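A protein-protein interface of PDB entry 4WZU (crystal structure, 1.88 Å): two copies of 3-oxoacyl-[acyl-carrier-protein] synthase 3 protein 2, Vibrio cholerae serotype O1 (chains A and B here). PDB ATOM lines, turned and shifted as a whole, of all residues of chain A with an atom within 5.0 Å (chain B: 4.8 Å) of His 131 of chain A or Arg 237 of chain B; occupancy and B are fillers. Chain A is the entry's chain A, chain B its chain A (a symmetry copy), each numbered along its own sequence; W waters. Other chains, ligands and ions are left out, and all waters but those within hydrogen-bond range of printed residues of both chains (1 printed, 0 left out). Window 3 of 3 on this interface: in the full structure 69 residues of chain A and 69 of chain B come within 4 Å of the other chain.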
ATOM      1  N   ASP A  75     -19.964  17.503 -24.719  1.00  0.00           N
ATOM      2  CA  ASP A  75     -20.932  17.658 -23.620  1.00  0.00           C
ATOM      3  C   ASP A  75     -22.272  17.044 -23.954  1.00  0.00           C
ATOM      4  O   ASP A  75     -23.126  16.931 -23.078  1.00  0.00           O
ATOM      5  CB  ASP A  75     -21.137  19.136 -23.267  1.00  0.00           C
ATOM      6  CG  ASP A  75     -19.920  19.762 -22.677  1.00  0.00           C
ATOM      7  OD1 ASP A  75     -19.143  19.044 -22.029  1.00  0.00           O
ATOM      8  OD2 ASP A  75     -19.722  20.981 -22.854  1.00  0.00           O
ATOM      9  N   LEU A 126     -29.917  23.656 -27.616  1.00  0.00           N
ATOM     10  CA  LEU A 126     -29.308  23.315 -26.298  1.00  0.00           C
ATOM     11  C   LEU A 126     -28.017  24.121 -26.069  1.00  0.00           C
ATOM     12  O   LEU A 126     -27.805  24.734 -25.016  1.00  0.00           O
ATOM     13  CB  LEU A 126     -29.043  21.806 -26.213  1.00  0.00           C
ATOM     14  CG  LEU A 126     -30.259  20.946 -25.916  1.00  0.00           C
ATOM     15  CD1 LEU A 126     -29.987  19.470 -26.228  1.00  0.00           C
ATOM     16  CD2 LEU A 126     -30.636  21.064 -24.450  1.00  0.00           C
ATOM     17  N   ALA A 129     -28.739  28.018 -25.647  1.00  0.00           N
ATOM     18  CA  ALA A 129     -29.396  28.485 -24.447  1.00  0.00           C
ATOM     19  C   ALA A 129     -28.745  27.987 -23.175  1.00  0.00           C
ATOM     20  O   ALA A 129     -29.143  28.425 -22.117  1.00  0.00           O
ATOM     21  CB  ALA A 129     -30.867  28.094 -24.460  1.00  0.00           C
ATOM     22  N   SER A 130     -27.812  27.044 -23.246  1.00  0.00           N
ATOM     23  CA  SER A 130     -27.181  26.546 -22.062  1.00  0.00           C
ATOM     24  C   SER A 130     -25.699  26.303 -22.272  1.00  0.00           C
ATOM     25  O   SER A 130     -25.084  26.903 -23.152  1.00  0.00           O
ATOM     26  CB  SER A 130     -27.901  25.298 -21.541  1.00  0.00           C
ATOM     27  OG  SER A 130     -27.664  25.146 -20.137  1.00  0.00           O
ATOM     28  N   HIS A 131     -25.110  25.482 -21.413  1.00  0.00           N
ATOM     29  CA  HIS A 131     -23.651  25.460 -21.266  1.00  0.00           C
ATOM     30  C   HIS A 131     -22.871  24.551 -22.223  1.00  0.00           C
ATOM     31  O   HIS A 131     -21.635  24.657 -22.255  1.00  0.00           O
ATOM     32  CB  HIS A 131     -23.245  25.161 -19.814  1.00  0.00           C
ATOM     33  CG  HIS A 131     -24.125  24.169 -19.127  1.00  0.00           C
ATOM     34  ND1 HIS A 131     -24.955  24.521 -18.079  1.00  0.00           N
ATOM     35  CD2 HIS A 131     -24.301  22.843 -19.325  1.00  0.00           C
ATOM     36  CE1 HIS A 131     -25.607  23.451 -17.669  1.00  0.00           C
ATOM     37  NE2 HIS A 131     -25.228  22.421 -18.411  1.00  0.00           N
ATOM     38  N   TYR A 132     -23.546  23.743 -23.037  1.00  0.00           N
ATOM     39  CA  TYR A 132     -22.909  22.710 -23.845  1.00  0.00           C
ATOM     40  C   TYR A 132     -21.897  23.337 -24.834  1.00  0.00           C
ATOM     41  O   TYR A 132     -22.251  24.201 -25.624  1.00  0.00           O
ATOM     42  CB  TYR A 132     -23.959  21.902 -24.616  1.00  0.00           C
ATOM     43  CG  TYR A 132     -25.094  21.364 -23.741  1.00  0.00           C
ATOM     44  CD1 TYR A 132     -26.213  22.142 -23.487  1.00  0.00           C
ATOM     45  CD2 TYR A 132     -25.010  20.096 -23.129  1.00  0.00           C
ATOM     46  CE1 TYR A 132     -27.227  21.679 -22.669  1.00  0.00           C
ATOM     47  CE2 TYR A 132     -26.025  19.619 -22.303  1.00  0.00           C
ATOM     48  CZ  TYR A 132     -27.134  20.411 -22.093  1.00  0.00           C
ATOM     49  OH  TYR A 132     -28.162  19.971 -21.291  1.00  0.00           O
ATOM     50  N   ARG A 133     -20.650  22.897 -24.765  1.00  0.00           N
ATOM     51  CA  ARG A 133     -19.551  23.541 -25.515  1.00  0.00           C
ATOM     52  C   ARG A 133     -19.404  22.872 -26.879  1.00  0.00           C
ATOM     53  O   ARG A 133     -19.137  23.537 -27.891  1.00  0.00           O
ATOM     54  CB  ARG A 133     -18.211  23.414 -24.775  1.00  0.00           C
ATOM     55  CG  ARG A 133     -18.144  23.800 -23.305  1.00  0.00           C
ATOM     56  CD  ARG A 133     -16.924  23.173 -22.616  1.00  0.00           C
ATOM     57  NE  ARG A 133     -17.052  21.713 -22.427  1.00  0.00           N
ATOM     58  CZ  ARG A 133     -16.232  20.960 -21.687  1.00  0.00           C
ATOM     59  NH1 ARG A 133     -15.175  21.504 -21.080  1.00  0.00           N
ATOM     60  NH2 ARG A 133     -16.447  19.646 -21.553  1.00  0.00           N
ATOM     61  N   LYS A 169     -19.336  25.497 -30.054  1.00  0.00           N
ATOM     62  CA  LYS A 169     -19.917  26.783 -29.753  1.00  0.00           C
ATOM     63  C   LYS A 169     -19.016  27.893 -30.245  1.00  0.00           C
ATOM     64  O   LYS A 169     -17.781  27.792 -30.178  1.00  0.00           O
ATOM     65  CB  LYS A 169     -20.223  26.901 -28.278  1.00  0.00           C
ATOM     66  CG  LYS A 169     -20.924  28.186 -27.905  1.00  0.00           C
ATOM     67  CD  LYS A 169     -21.264  28.176 -26.428  1.00  0.00           C
ATOM     68  CE  LYS A 169     -22.571  27.481 -26.222  1.00  0.00           C
ATOM     69  NZ  LYS A 169     -23.068  27.508 -24.831  1.00  0.00           N
ATOM     70  N   ASP B 178     -31.378  26.449 -14.112  1.00  0.00           N
ATOM     71  CA  ASP B 178     -30.248  25.624 -14.509  1.00  0.00           C
ATOM     72  C   ASP B 178     -30.567  24.120 -14.422  1.00  0.00           C
ATOM     73  O   ASP B 178     -31.433  23.711 -13.670  1.00  0.00           O
ATOM     74  CB  ASP B 178     -29.045  25.990 -13.692  1.00  0.00           C
ATOM     75  CG  ASP B 178     -27.764  25.437 -14.272  1.00  0.00           C
ATOM     76  OD1 ASP B 178     -27.662  25.210 -15.512  1.00  0.00           O
ATOM     77  OD2 ASP B 178     -26.886  25.165 -13.445  1.00  0.00           O
ATOM     78  N   ALA B 179     -29.917  23.329 -15.274  1.00  0.00           N
ATOM     79  CA  ALA B 179     -30.021  21.868 -15.278  1.00  0.00           C
ATOM     80  C   ALA B 179     -28.683  21.296 -15.728  1.00  0.00           C
ATOM     81  O   ALA B 179     -27.976  21.915 -16.542  1.00  0.00           O
ATOM     82  CB  ALA B 179     -31.122  21.380 -16.197  1.00  0.00           C
ATOM     83  N   GLN B 180     -28.325  20.154 -15.143  1.00  0.00           N
ATOM     84  CA  GLN B 180     -27.193  19.403 -15.573  1.00  0.00           C
ATOM     85  C   GLN B 180     -27.656  17.979 -15.818  1.00  0.00           C
ATOM     86  O   GLN B 180     -28.050  17.259 -14.887  1.00  0.00           O
ATOM     87  CB  GLN B 180     -26.093  19.413 -14.533  1.00  0.00           C
ATOM     88  CG  GLN B 180     -24.767  18.873 -15.062  1.00  0.00           C
ATOM     89  CD  GLN B 180     -24.105  19.791 -16.079  1.00  0.00           C
ATOM     90  OE1 GLN B 180     -24.200  21.009 -16.001  1.00  0.00           O
ATOM     91  NE2 GLN B 180     -23.419  19.199 -17.040  1.00  0.00           N
ATOM     92  N   GLN B 233     -23.941  20.640  -8.812  1.00  0.00           N
ATOM     93  CA  GLN B 233     -23.662  21.594  -9.876  1.00  0.00           C
ATOM     94  C   GLN B 233     -24.809  22.619 -10.044  1.00  0.00           C
ATOM     95  O   GLN B 233     -24.561  23.822 -10.157  1.00  0.00           O
ATOM     96  CB  GLN B 233     -23.432  20.866 -11.206  1.00  0.00           C
ATOM     97  CG  GLN B 233     -22.143  20.063 -11.284  1.00  0.00           C
ATOM     98  CD  GLN B 233     -21.907  19.537 -12.695  1.00  0.00           C
ATOM     99  OE1 GLN B 233     -21.906  18.336 -12.947  1.00  0.00           O
ATOM    100  NE2 GLN B 233     -21.716  20.448 -13.620  1.00  0.00           N
ATOM    101  N   VAL B 234     -26.042  22.131 -10.073  1.00  0.00           N
ATOM    102  CA  VAL B 234     -27.202  23.013 -10.221  1.00  0.00           C
ATOM    103  C   VAL B 234     -27.307  23.979  -9.046  1.00  0.00           C
ATOM    104  O   VAL B 234     -27.488  25.181  -9.259  1.00  0.00           O
ATOM    105  CB  VAL B 234     -28.486  22.197 -10.392  1.00  0.00           C
ATOM    106  CG1 VAL B 234     -29.719  23.060 -10.231  1.00  0.00           C
ATOM    107  CG2 VAL B 234     -28.495  21.485 -11.734  1.00  0.00           C
ATOM    108  N   LEU B 235     -27.126  23.473  -7.820  1.00  0.00           N
ATOM    109  CA  LEU B 235     -27.123  24.348  -6.646  1.00  0.00           C
ATOM    110  C   LEU B 235     -26.056  25.414  -6.723  1.00  0.00           C
ATOM    111  O   LEU B 235     -26.346  26.581  -6.504  1.00  0.00           O
ATOM    112  CB  LEU B 235     -26.923  23.557  -5.371  1.00  0.00           C
ATOM    113  CG  LEU B 235     -28.138  22.762  -4.941  1.00  0.00           C
ATOM    114  CD1 LEU B 235     -27.738  21.755  -3.866  1.00  0.00           C
ATOM    115  CD2 LEU B 235     -29.186  23.733  -4.403  1.00  0.00           C
ATOM    116  N   ALA B 236     -24.825  25.003  -7.039  1.00  0.00           N
ATOM    117  CA  ALA B 236     -23.714  25.928  -7.123  1.00  0.00           C
ATOM    118  C   ALA B 236     -23.957  27.009  -8.175  1.00  0.00           C
ATOM    119  O   ALA B 236     -23.768  28.204  -7.909  1.00  0.00           O
ATOM    120  CB  ALA B 236     -22.404  25.199  -7.393  1.00  0.00           C
ATOM    121  N   ARG B 237     -24.407  26.605  -9.357  1.00  0.00           N
ATOM    122  CA  ARG B 237     -24.619  27.576 -10.419  1.00  0.00           C
ATOM    123  C   ARG B 237     -25.801  28.526 -10.165  1.00  0.00           C
ATOM    124  O   ARG B 237     -25.805  29.668 -10.633  1.00  0.00           O
ATOM    125  CB  ARG B 237     -24.730  26.861 -11.784  1.00  0.00           C
ATOM    126  CG  ARG B 237     -23.369  26.392 -12.288  1.00  0.00           C
ATOM    127  CD  ARG B 237     -23.350  26.061 -13.774  1.00  0.00           C
ATOM    128  NE  ARG B 237     -24.420  25.132 -14.088  1.00  0.00           N
ATOM    129  CZ  ARG B 237     -24.272  23.849 -14.431  1.00  0.00           C
ATOM    130  NH1 ARG B 237     -23.096  23.285 -14.614  1.00  0.00           N
ATOM    131  NH2 ARG B 237     -25.345  23.134 -14.683  1.00  0.00           N
ATOM    132  N   SER B 238     -26.799  28.039  -9.430  1.00  0.00           N
ATOM    133  CA  SER B 238     -28.013  28.805  -9.132  1.00  0.00           C
ATOM    134  C   SER B 238     -27.765  29.921  -8.113  1.00  0.00           C
ATOM    135  O   SER B 238     -28.486  30.910  -8.078  1.00  0.00           O
ATOM    136  CB  SER B 238     -29.115  27.877  -8.594  1.00  0.00           C
ATOM    137  OG  SER B 238     -28.951  27.568  -7.204  1.00  0.00           O
ATOM    138  N   GLY B 239     -26.748  29.744  -7.284  1.00  0.00           N
ATOM    139  CA  GLY B 239     -26.515  30.619  -6.125  1.00  0.00           C
ATOM    140  C   GLY B 239     -27.562  30.440  -5.029  1.00  0.00           C
ATOM    141  O   GLY B 239     -27.801  31.356  -4.253  1.00  0.00           O
HETATM  142  O   HOH W   1     -28.611  23.007 -18.996  1.00  0.00           O
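NE2 of His 131 of chain A sits close to O of Ala 179 of chain B, 3.4 Å away.
A ring nitrogen (NE2) of His 131 of chain A lies within hydrogen-bond range of the side-chain amide oxygen (OE1) of Gln 180 of chain B (3.0 Å).
A ring nitrogen (ND1) of His 131 of chain A sits at hydrogen-bond distance from the side-chain hydroxyl of Ser 130 of chain A (3.5 Å).
The side-chain carboxylate of Asp 178 of chain B is in salt-bridge range of the guanidinium group of Arg 237 of chain B (2.5 Å).
The backbone carbonyl oxygen (O) of Ala 179 of chain B sits at hydrogen-bond distance from the guanidinium group (NH2) of Arg 237 of chain B, at 3.4 Å.
The side-chain amide oxygen (OE1) of Gln 180 of chain B is in hydrogen-bond range of the side-chain amide nitrogen (NE2) of Gln 233 of chain B.
NH2 of Arg 237 of chain B lies within hydrogen-bond range of OE1 of Gln 180 of chain B (2.8 Å).
The guanidinium group (NH1) of Arg 237 of chain B sits close to the side-chain amide nitrogen (NE2) of Gln 233 of chain B (3.3 Å).
Among the printed residues, merely in contact across the chains: His 131 of chain A with Asp 178 of chain B and His 131 of chain A with Arg 237 of chain B.
Printed residues of chain A within 4 Å of Asp 178 of chain B: His 131.
Printed residues of chain A within 4 Å of Ala 179 of chain B: His 131.
Of the printed residues of chain A, Gln 180 of chain B touches His 131.
Arg 237 of chain B touches one residue of chain A.
The nearest printed residue of chain A that does not touch Asp 178 of chain B is Ser 130 of chain A (4.6 Å).
Among the printed residues, no Asp or Glu carboxylate lies within 4 Å of a Lys or Arg side-chain nitrogen of the other chain.
No position is printed for both chains.
Of the 4 pairs that touch across the chains among the printed residues, none has its exchanged pair printed and touching as well.
Water W1 lies within hydrogen-bond range of OG of Ser 130 of chain A, O of Ala 179 of chain B and NE2 of His 131 of chain A.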
